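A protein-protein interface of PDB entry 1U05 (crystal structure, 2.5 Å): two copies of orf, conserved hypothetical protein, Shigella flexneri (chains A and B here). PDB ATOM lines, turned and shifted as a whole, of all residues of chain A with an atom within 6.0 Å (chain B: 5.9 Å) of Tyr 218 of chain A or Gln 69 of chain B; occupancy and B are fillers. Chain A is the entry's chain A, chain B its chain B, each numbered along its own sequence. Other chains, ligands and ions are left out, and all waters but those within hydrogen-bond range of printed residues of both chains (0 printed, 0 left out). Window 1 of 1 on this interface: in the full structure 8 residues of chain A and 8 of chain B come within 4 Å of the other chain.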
ATOM      1  N   ASP A 106      27.656  21.102 -15.110  1.00  0.00           N
ATOM      2  CA  ASP A 106      27.079  22.456 -15.040  1.00  0.00           C
ATOM      3  C   ASP A 106      26.792  23.009 -16.440  1.00  0.00           C
ATOM      4  O   ASP A 106      25.712  23.548 -16.707  1.00  0.00           O
ATOM      5  CB  ASP A 106      27.988  23.460 -14.313  1.00  0.00           C
ATOM      6  CG  ASP A 106      27.783  23.461 -12.808  1.00  0.00           C
ATOM      7  OD1 ASP A 106      26.646  23.242 -12.354  1.00  0.00           O
ATOM      8  OD2 ASP A 106      28.760  23.701 -12.075  1.00  0.00           O
ATOM      9  N   ALA A 156      21.806  21.020 -16.422  1.00  0.00           N
ATOM     10  CA  ALA A 156      22.883  21.984 -16.347  1.00  0.00           C
ATOM     11  C   ALA A 156      22.555  22.841 -15.141  1.00  0.00           C
ATOM     12  O   ALA A 156      21.549  22.600 -14.477  1.00  0.00           O
ATOM     13  CB  ALA A 156      22.913  22.831 -17.609  1.00  0.00           C
ATOM     14  N   ILE A 157      23.399  23.826 -14.851  1.00  0.00           N
ATOM     15  CA  ILE A 157      23.148  24.722 -13.732  1.00  0.00           C
ATOM     16  C   ILE A 157      21.984  25.658 -14.101  1.00  0.00           C
ATOM     17  O   ILE A 157      22.020  26.344 -15.126  1.00  0.00           O
ATOM     18  CB  ILE A 157      24.409  25.531 -13.389  1.00  0.00           C
ATOM     19  CG1 ILE A 157      24.100  26.488 -12.241  1.00  0.00           C
ATOM     20  CG2 ILE A 157      24.927  26.260 -14.635  1.00  0.00           C
ATOM     21  CD1 ILE A 157      25.315  27.079 -11.608  1.00  0.00           C
ATOM     22  N   GLY A 158      20.946  25.661 -13.267  1.00  0.00           N
ATOM     23  CA  GLY A 158      19.763  26.469 -13.530  1.00  0.00           C
ATOM     24  C   GLY A 158      19.842  27.976 -13.306  1.00  0.00           C
ATOM     25  O   GLY A 158      20.843  28.491 -12.798  1.00  0.00           O
ATOM     26  N   ALA A 161      21.092  29.406  -9.906  1.00  0.00           N
ATOM     27  CA  ALA A 161      22.452  29.187  -9.442  1.00  0.00           C
ATOM     28  C   ALA A 161      23.510  29.660 -10.439  1.00  0.00           C
ATOM     29  O   ALA A 161      24.661  29.892 -10.067  1.00  0.00           O
ATOM     30  CB  ALA A 161      22.651  27.704  -9.121  1.00  0.00           C
ATOM     31  N   CYS A 216      18.639  21.141 -12.628  1.00  0.00           N
ATOM     32  CA  CYS A 216      19.665  22.044 -12.142  1.00  0.00           C
ATOM     33  C   CYS A 216      20.749  21.233 -11.450  1.00  0.00           C
ATOM     34  O   CYS A 216      20.533  20.693 -10.365  1.00  0.00           O
ATOM     35  CB  CYS A 216      19.070  23.066 -11.175  1.00  0.00           C
ATOM     36  SG  CYS A 216      20.250  24.339 -10.633  1.00  0.00           S
ATOM     37  N   THR A 217      21.911  21.140 -12.091  1.00  0.00           N
ATOM     38  CA  THR A 217      23.031  20.388 -11.539  1.00  0.00           C
ATOM     39  C   THR A 217      23.454  20.912 -10.167  1.00  0.00           C
ATOM     40  O   THR A 217      23.829  20.140  -9.290  1.00  0.00           O
ATOM     41  CB  THR A 217      24.268  20.453 -12.462  1.00  0.00           C
ATOM     42  OG1 THR A 217      24.706  21.809 -12.565  1.00  0.00           O
ATOM     43  CG2 THR A 217      23.943  19.924 -13.843  1.00  0.00           C
ATOM     44  N   TYR A 218      23.390  22.228  -9.992  1.00  0.00           N
ATOM     45  CA  TYR A 218      23.782  22.871  -8.740  1.00  0.00           C
ATOM     46  C   TYR A 218      22.852  22.538  -7.565  1.00  0.00           C
ATOM     47  O   TYR A 218      23.302  22.091  -6.505  1.00  0.00           O
ATOM     48  CB  TYR A 218      23.826  24.387  -8.941  1.00  0.00           C
ATOM     49  CG  TYR A 218      24.439  25.136  -7.784  1.00  0.00           C
ATOM     50  CD1 TYR A 218      25.784  25.502  -7.804  1.00  0.00           C
ATOM     51  CD2 TYR A 218      23.689  25.431  -6.638  1.00  0.00           C
ATOM     52  CE1 TYR A 218      26.367  26.136  -6.722  1.00  0.00           C
ATOM     53  CE2 TYR A 218      24.267  26.061  -5.548  1.00  0.00           C
ATOM     54  CZ  TYR A 218      25.607  26.411  -5.598  1.00  0.00           C
ATOM     55  OH  TYR A 218      26.189  27.049  -4.532  1.00  0.00           O
ATOM     56  N   THR A 219      21.557  22.770  -7.775  1.00  0.00           N
ATOM     57  CA  THR A 219      20.510  22.540  -6.780  1.00  0.00           C
ATOM     58  C   THR A 219      20.300  21.066  -6.385  1.00  0.00           C
ATOM     59  O   THR A 219      20.301  20.726  -5.198  1.00  0.00           O
ATOM     60  CB  THR A 219      19.149  23.090  -7.292  1.00  0.00           C
ATOM     61  OG1 THR A 219      19.331  24.409  -7.831  1.00  0.00           O
ATOM     62  CG2 THR A 219      18.123  23.137  -6.157  1.00  0.00           C
ATOM     63  N   GLU A 220      20.101  20.203  -7.379  1.00  0.00           N
ATOM     64  CA  GLU A 220      19.865  18.782  -7.135  1.00  0.00           C
ATOM     65  C   GLU A 220      21.181  18.051  -6.911  1.00  0.00           C
ATOM     66  O   GLU A 220      21.555  17.158  -7.681  1.00  0.00           O
ATOM     67  CB  GLU A 220      19.126  18.183  -8.322  1.00  0.00           C
ATOM     68  CG  GLU A 220      18.079  19.132  -8.896  1.00  0.00           C
ATOM     69  CD  GLU A 220      17.117  18.451  -9.833  1.00  0.00           C
ATOM     70  OE1 GLU A 220      16.310  17.642  -9.341  1.00  0.00           O
ATOM     71  OE2 GLU A 220      17.166  18.716 -11.054  1.00  0.00           O
ATOM     72  N   ASN A 221      21.869  18.436  -5.838  1.00  0.00           N
ATOM     73  CA  ASN A 221      23.164  17.865  -5.497  1.00  0.00           C
ATOM     74  C   ASN A 221      23.159  16.362  -5.238  1.00  0.00           C
ATOM     75  O   ASN A 221      24.213  15.717  -5.262  1.00  0.00           O
ATOM     76  CB  ASN A 221      23.769  18.623  -4.307  1.00  0.00           C
ATOM     77  CG  ASN A 221      22.856  18.659  -3.108  1.00  0.00           C
ATOM     78  OD1 ASN A 221      22.779  17.696  -2.347  1.00  0.00           O
ATOM     79  ND2 ASN A 221      22.156  19.772  -2.929  1.00  0.00           N
ATOM     80  N   PHE A 224      23.253  15.217  -9.336  1.00  0.00           N
ATOM     81  CA  PHE A 224      24.291  15.662 -10.260  1.00  0.00           C
ATOM     82  C   PHE A 224      25.551  16.207  -9.609  1.00  0.00           C
ATOM     83  O   PHE A 224      25.566  16.572  -8.433  1.00  0.00           O
ATOM     84  CB  PHE A 224      23.741  16.771 -11.172  1.00  0.00           C
ATOM     85  CG  PHE A 224      22.458  16.422 -11.858  1.00  0.00           C
ATOM     86  CD1 PHE A 224      22.422  15.435 -12.847  1.00  0.00           C
ATOM     87  CD2 PHE A 224      21.273  17.071 -11.508  1.00  0.00           C
ATOM     88  CE1 PHE A 224      21.225  15.094 -13.475  1.00  0.00           C
ATOM     89  CE2 PHE A 224      20.063  16.742 -12.126  1.00  0.00           C
ATOM     90  CZ  PHE A 224      20.037  15.751 -13.112  1.00  0.00           C
ATOM     91  N   PHE A 225      26.607  16.276 -10.405  1.00  0.00           N
ATOM     92  CA  PHE A 225      27.867  16.849  -9.962  1.00  0.00           C
ATOM     93  C   PHE A 225      27.722  18.308 -10.375  1.00  0.00           C
ATOM     94  O   PHE A 225      26.919  18.629 -11.242  1.00  0.00           O
ATOM     95  CB  PHE A 225      29.047  16.228 -10.709  1.00  0.00           C
ATOM     96  CG  PHE A 225      29.281  14.779 -10.393  1.00  0.00           C
ATOM     97  CD1 PHE A 225      29.680  14.383  -9.117  1.00  0.00           C
ATOM     98  CD2 PHE A 225      29.137  13.804 -11.386  1.00  0.00           C
ATOM     99  CE1 PHE A 225      29.938  13.023  -8.832  1.00  0.00           C
ATOM    100  CE2 PHE A 225      29.391  12.444 -11.115  1.00  0.00           C
ATOM    101  CZ  PHE A 225      29.792  12.052  -9.836  1.00  0.00           C
ATOM    102  N   SER A 226      28.485  19.196  -9.760  1.00  0.00           N
ATOM    103  CA  SER A 226      28.413  20.611 -10.099  1.00  0.00           C
ATOM    104  C   SER A 226      29.754  21.261  -9.832  1.00  0.00           C
ATOM    105  O   SER A 226      30.202  21.321  -8.692  1.00  0.00           O
ATOM    106  CB  SER A 226      27.325  21.302  -9.272  1.00  0.00           C
ATOM    107  OG  SER A 226      27.509  22.710  -9.273  1.00  0.00           O
ATOM    108  N   ARG A 228      30.469  24.382 -10.167  1.00  0.00           N
ATOM    109  CA  ARG A 228      30.265  25.625  -9.443  1.00  0.00           C
ATOM    110  C   ARG A 228      30.134  25.338  -7.951  1.00  0.00           C
ATOM    111  O   ARG A 228      30.683  26.046  -7.121  1.00  0.00           O
ATOM    112  CB  ARG A 228      28.996  26.321  -9.942  1.00  0.00           C
ATOM    113  CG  ARG A 228      28.786  27.712  -9.378  1.00  0.00           C
ATOM    114  CD  ARG A 228      29.833  28.673  -9.923  1.00  0.00           C
ATOM    115  NE  ARG A 228      29.678  28.911 -11.359  1.00  0.00           N
ATOM    116  CZ  ARG A 228      28.767  29.719 -11.900  1.00  0.00           C
ATOM    117  NH1 ARG A 228      27.911  30.387 -11.132  1.00  0.00           N
ATOM    118  NH2 ARG A 228      28.710  29.856 -13.216  1.00  0.00           N
ATOM    119  N   ARG A 229      29.413  24.274  -7.628  1.00  0.00           N
ATOM    120  CA  ARG A 229      29.169  23.892  -6.250  1.00  0.00           C
ATOM    121  C   ARG A 229      30.335  23.215  -5.537  1.00  0.00           C
ATOM    122  O   ARG A 229      30.672  23.578  -4.412  1.00  0.00           O
ATOM    123  CB  ARG A 229      27.947  22.966  -6.200  1.00  0.00           C
ATOM    124  CG  ARG A 229      27.455  22.619  -4.800  1.00  0.00           C
ATOM    125  CD  ARG A 229      26.352  21.581  -4.879  1.00  0.00           C
ATOM    126  NE  ARG A 229      26.871  20.329  -5.416  1.00  0.00           N
ATOM    127  CZ  ARG A 229      26.241  19.565  -6.299  1.00  0.00           C
ATOM    128  NH1 ARG A 229      25.055  19.914  -6.760  1.00  0.00           N
ATOM    129  NH2 ARG A 229      26.809  18.446  -6.725  1.00  0.00           N
ATOM    130  N   TRP B  66      24.582  35.482   5.491  1.00  0.00           N
ATOM    131  CA  TRP B  66      24.231  34.353   4.648  1.00  0.00           C
ATOM    132  C   TRP B  66      25.457  33.797   3.952  1.00  0.00           C
ATOM    133  O   TRP B  66      26.269  34.545   3.409  1.00  0.00           O
ATOM    134  CB  TRP B  66      23.184  34.770   3.611  1.00  0.00           C
ATOM    135  CG  TRP B  66      21.882  35.164   4.218  1.00  0.00           C
ATOM    136  CD1 TRP B  66      21.256  36.369   4.103  1.00  0.00           C
ATOM    137  CD2 TRP B  66      21.043  34.354   5.042  1.00  0.00           C
ATOM    138  NE1 TRP B  66      20.074  36.364   4.808  1.00  0.00           N
ATOM    139  CE2 TRP B  66      19.918  35.138   5.395  1.00  0.00           C
ATOM    140  CE3 TRP B  66      21.128  33.039   5.520  1.00  0.00           C
ATOM    141  CZ2 TRP B  66      18.890  34.653   6.202  1.00  0.00           C
ATOM    142  CZ3 TRP B  66      20.104  32.556   6.327  1.00  0.00           C
ATOM    143  CH2 TRP B  66      19.000  33.365   6.658  1.00  0.00           C
ATOM    144  N   LEU B  67      25.584  32.479   3.989  1.00  0.00           N
ATOM    145  CA  LEU B  67      26.694  31.790   3.356  1.00  0.00           C
ATOM    146  C   LEU B  67      26.223  31.295   2.002  1.00  0.00           C
ATOM    147  O   LEU B  67      25.058  31.466   1.645  1.00  0.00           O
ATOM    148  CB  LEU B  67      27.102  30.566   4.174  1.00  0.00           C
ATOM    149  CG  LEU B  67      27.494  30.737   5.635  1.00  0.00           C
ATOM    150  CD1 LEU B  67      27.744  29.349   6.213  1.00  0.00           C
ATOM    151  CD2 LEU B  67      28.745  31.652   5.766  1.00  0.00           C
ATOM    152  N   GLU B  68      27.149  30.703   1.250  1.00  0.00           N
ATOM    153  CA  GLU B  68      26.844  30.089  -0.035  1.00  0.00           C
ATOM    154  C   GLU B  68      26.958  28.627   0.329  1.00  0.00           C
ATOM    155  O   GLU B  68      28.020  28.031   0.178  1.00  0.00           O
ATOM    156  CB  GLU B  68      27.893  30.395  -1.109  1.00  0.00           C
ATOM    157  CG  GLU B  68      27.810  31.780  -1.729  1.00  0.00           C
ATOM    158  CD  GLU B  68      28.666  31.907  -2.990  1.00  0.00           C
ATOM    159  OE1 GLU B  68      28.923  33.058  -3.417  1.00  0.00           O
ATOM    160  OE2 GLU B  68      29.071  30.860  -3.554  1.00  0.00           O
ATOM    161  N   GLN B  69      25.875  28.066   0.850  1.00  0.00           N
ATOM    162  CA  GLN B  69      25.872  26.665   1.251  1.00  0.00           C
ATOM    163  C   GLN B  69      25.993  25.747   0.037  1.00  0.00           C
ATOM    164  O   GLN B  69      25.179  25.798  -0.885  1.00  0.00           O
ATOM    165  CB  GLN B  69      24.602  26.366   2.056  1.00  0.00           C
ATOM    166  CG  GLN B  69      24.655  26.923   3.481  1.00  0.00           C
ATOM    167  CD  GLN B  69      23.279  27.244   4.056  1.00  0.00           C
ATOM    168  OE1 GLN B  69      22.298  26.551   3.778  1.00  0.00           O
ATOM    169  NE2 GLN B  69      23.208  28.290   4.873  1.00  0.00           N
ATOM    170  N   VAL B  70      27.027  24.916   0.038  1.00  0.00           N
ATOM    171  CA  VAL B  70      27.257  24.010  -1.076  1.00  0.00           C
ATOM    172  C   VAL B  70      27.227  22.556  -0.629  1.00  0.00           C
ATOM    173  O   VAL B  70      27.632  21.656  -1.363  1.00  0.00           O
ATOM    174  CB  VAL B  70      28.610  24.326  -1.754  1.00  0.00           C
ATOM    175  CG1 VAL B  70      28.568  25.736  -2.342  1.00  0.00           C
ATOM    176  CG2 VAL B  70      29.753  24.204  -0.750  1.00  0.00           C
ATOM    177  N   HIS B  71      26.726  22.345   0.584  1.00  0.00           N
ATOM    178  CA  HIS B  71      26.630  21.024   1.189  1.00  0.00           C
ATOM    179  C   HIS B  71      27.979  20.379   1.414  1.00  0.00           C
ATOM    180  O   HIS B  71      28.111  19.157   1.392  1.00  0.00           O
ATOM    181  CB  HIS B  71      25.733  20.106   0.363  1.00  0.00           C
ATOM    182  CG  HIS B  71      24.284  20.451   0.470  1.00  0.00           C
ATOM    183  ND1 HIS B  71      23.724  21.530  -0.183  1.00  0.00           N
ATOM    184  CD2 HIS B  71      23.287  19.890   1.193  1.00  0.00           C
ATOM    185  CE1 HIS B  71      22.443  21.615   0.131  1.00  0.00           C
ATOM    186  NE2 HIS B  71      22.154  20.630   0.963  1.00  0.00           N
ATOM    187  N   GLY B  72      28.981  21.219   1.642  1.00  0.00           N
ATOM    188  CA  GLY B  72      30.307  20.718   1.907  1.00  0.00           C
ATOM    189  C   GLY B  72      30.465  20.585   3.405  1.00  0.00           C
ATOM    190  O   GLY B  72      29.534  20.198   4.111  1.00  0.00           O
ATOM    191  N   LYS B  86      32.613  33.149   0.380  1.00  0.00           N
ATOM    192  CA  LYS B  86      31.500  32.976   1.291  1.00  0.00           C
ATOM    193  C   LYS B  86      31.016  31.528   1.229  1.00  0.00           C
ATOM    194  O   LYS B  86      30.140  31.127   1.993  1.00  0.00           O
ATOM    195  CB  LYS B  86      30.380  33.947   0.914  1.00  0.00           C
ATOM    196  CG  LYS B  86      29.367  34.183   2.010  1.00  0.00           C
ATOM    197  CD  LYS B  86      29.106  35.674   2.235  1.00  0.00           C
ATOM    198  CE  LYS B  86      30.285  36.364   2.912  1.00  0.00           C
ATOM    199  NZ  LYS B  86      29.957  37.775   3.278  1.00  0.00           N
ATOM    200  N   ARG B  87      31.608  30.753   0.319  1.00  0.00           N
ATOM    201  CA  ARG B  87      31.266  29.339   0.137  1.00  0.00           C
ATOM    202  C   ARG B  87      31.580  28.538   1.396  1.00  0.00           C
ATOM    203  O   ARG B  87      32.746  28.305   1.712  1.00  0.00           O
ATOM    204  CB  ARG B  87      32.055  28.732  -1.044  1.00  0.00           C
ATOM    205  CG  ARG B  87      31.620  29.204  -2.429  1.00  0.00           C
ATOM    206  CD  ARG B  87      32.397  28.526  -3.579  1.00  0.00           C
ATOM    207  NE  ARG B  87      32.184  27.073  -3.667  1.00  0.00           N
ATOM    208  CZ  ARG B  87      32.881  26.167  -2.980  1.00  0.00           C
ATOM    209  NH1 ARG B  87      33.843  26.557  -2.151  1.00  0.00           N
ATOM    210  NH2 ARG B  87      32.621  24.871  -3.120  1.00  0.00           N
ATOM    211  N   ALA B  88      30.543  28.108   2.108  1.00  0.00           N
ATOM    212  CA  ALA B  88      30.734  27.328   3.329  1.00  0.00           C
ATOM    213  C   ALA B  88      29.395  26.816   3.828  1.00  0.00           C
ATOM    214  O   ALA B  88      28.351  27.224   3.334  1.00  0.00           O
ATOM    215  CB  ALA B  88      31.407  28.184   4.405  1.00  0.00           C
ATOM    216  N   ASP B  89      29.423  25.917   4.801  1.00  0.00           N
ATOM    217  CA  ASP B  89      28.190  25.367   5.350  1.00  0.00           C
ATOM    218  C   ASP B  89      28.160  25.526   6.864  1.00  0.00           C
ATOM    219  O   ASP B  89      27.298  24.989   7.547  1.00  0.00           O
ATOM    220  CB  ASP B  89      28.052  23.899   4.948  1.00  0.00           C
ATOM    221  CG  ASP B  89      27.836  23.730   3.460  1.00  0.00           C
ATOM    222  OD1 ASP B  89      26.674  23.828   3.011  1.00  0.00           O
ATOM    223  OD2 ASP B  89      28.831  23.520   2.732  1.00  0.00           O
ATOM    224  N   ALA B 101      24.192  32.358  10.712  1.00  0.00           N
ATOM    225  CA  ALA B 101      22.930  31.813  10.242  1.00  0.00           C
ATOM    226  C   ALA B 101      23.099  30.728   9.190  1.00  0.00           C
ATOM    227  O   ALA B 101      24.028  30.766   8.380  1.00  0.00           O
ATOM    228  CB  ALA B 101      22.069  32.928   9.695  1.00  0.00           C
ATOM    229  N   VAL B 102      22.191  29.756   9.221  1.00  0.00           N
ATOM    230  CA  VAL B 102      22.198  28.658   8.265  1.00  0.00           C
ATOM    231  C   VAL B 102      20.783  28.444   7.740  1.00  0.00           C
ATOM    232  O   VAL B 102      19.832  28.327   8.507  1.00  0.00           O
ATOM    233  CB  VAL B 102      22.745  27.350   8.896  1.00  0.00           C
ATOM    234  CG1 VAL B 102      24.263  27.452   9.065  1.00  0.00           C
ATOM    235  CG2 VAL B 102      22.083  27.093  10.241  1.00  0.00           C
ATOM    236  N   MET B 103      20.662  28.413   6.421  1.00  0.00           N
ATOM    237  CA  MET B 103      19.382  28.246   5.736  1.00  0.00           C
ATOM    238  C   MET B 103      19.077  26.774   5.407  1.00  0.00           C
ATOM    239  O   MET B 103      19.867  26.107   4.743  1.00  0.00           O
ATOM    240  CB  MET B 103      19.418  29.081   4.458  1.00  0.00           C
ATOM    241  CG  MET B 103      18.081  29.335   3.826  1.00  0.00           C
ATOM    242  SD  MET B 103      18.276  30.629   2.613  1.00  0.00           S
ATOM    243  CE  MET B 103      18.016  32.093   3.629  1.00  0.00           C
ATOM    244  N   THR B 104      17.925  26.275   5.852  1.00  0.00           N
ATOM    245  CA  THR B 104      17.578  24.868   5.615  1.00  0.00           C
ATOM    246  C   THR B 104      16.123  24.568   5.266  1.00  0.00           C
ATOM    247  O   THR B 104      15.258  25.449   5.266  1.00  0.00           O
ATOM    248  CB  THR B 104      17.922  23.997   6.849  1.00  0.00           C
ATOM    249  OG1 THR B 104      17.109  24.397   7.957  1.00  0.00           O
ATOM    250  CG2 THR B 104      19.380  24.169   7.234  1.00  0.00           C
ATOM    251  N   HIS B 124      25.067  24.095   8.721  1.00  0.00           N
ATOM    252  CA  HIS B 124      24.078  23.496   7.838  1.00  0.00           C
ATOM    253  C   HIS B 124      24.682  22.136   7.519  1.00  0.00           C
ATOM    254  O   HIS B 124      25.576  22.027   6.681  1.00  0.00           O
ATOM    255  CB  HIS B 124      23.924  24.320   6.558  1.00  0.00           C
ATOM    256  CG  HIS B 124      23.409  23.532   5.391  1.00  0.00           C
ATOM    257  ND1 HIS B 124      24.207  23.166   4.331  1.00  0.00           N
ATOM    258  CD2 HIS B 124      22.177  23.037   5.121  1.00  0.00           C
ATOM    259  CE1 HIS B 124      23.491  22.486   3.455  1.00  0.00           C
ATOM    260  NE2 HIS B 124      22.256  22.392   3.911  1.00  0.00           N
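The backbone carbonyl oxygen of Arg 229 of chain A sits at hydrogen-bond distance from the guanidinium group of Arg 87 of chain B, 2.7 Å away.
The backbone carbonyl oxygen (O) of Ala 161 of chain A is in hydrogen-bond range of the guanidinium group (NH1) of Arg 228 of chain A (3.5 Å).
O of Tyr 218 of chain A sits at hydrogen-bond distance from NH1 of Arg 229 of chain A (2.8 Å).
O of Phe 224 of chain A sits at hydrogen-bond distance from NH2 of Arg 229 of chain A, 2.8 Å away.
OG of Ser 226 of chain A lies within hydrogen-bond range of N of Arg 229 of chain A (3.0 Å).
OE1 of Gln 69 of chain B sits close to O of Met 103 of chain B.
The backbone NH (N) of Val 70 of chain B lies within hydrogen-bond range of the side-chain carboxylate (OD1) of Asp 89 of chain B (3.2 Å).
Among the printed residues, pairs that only touch across the chains: Tyr 218 of chain A with Gln 69 of chain B (3.99 Å), Tyr 218 of chain A with Val 70 of chain B (3.5 Å), Asn 221 of chain A with His 71 of chain B (3.6 Å), Arg 228 of chain A with Arg 87 of chain B (3.9 Å) and Arg 229 of chain A with Val 70 of chain B (3.4 Å).
Of the printed residues of chain B, Tyr 218 of chain A touches Gln 69 and Val 70.
Of the printed residues of chain A, Arg 87 of chain B touches Arg 228 (3.9 Å) and Arg 229 (2.7 Å).
Of the printed residues of chain B, Arg 229 of chain A touches Val 70 (3.4 Å) and Arg 87 (2.7 Å).
Of the printed residues of chain A, His 71 of chain B touches Asn 221 (3.6 Å).
Thr 104 of chain B touches none of the printed residues of chain A.
Lys 86 of chain B touches none of the printed residues of chain A.
Printed residues of chain B that touch a printed residue of chain A: Gln 69, Val 70, His 71 and Arg 87.
Hydrophobic or aromatic side chains of chain B within 4 Å of the printed part of chain A: Val 70 and His 71.
Hydrophobic or aromatic side chains of chain A that line the printed part of chain B: Tyr 218.
No position is printed for both chains.
Of the 6 pairs that touch across the chains among the printed residues, none has its exchanged pair printed and touching as well.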
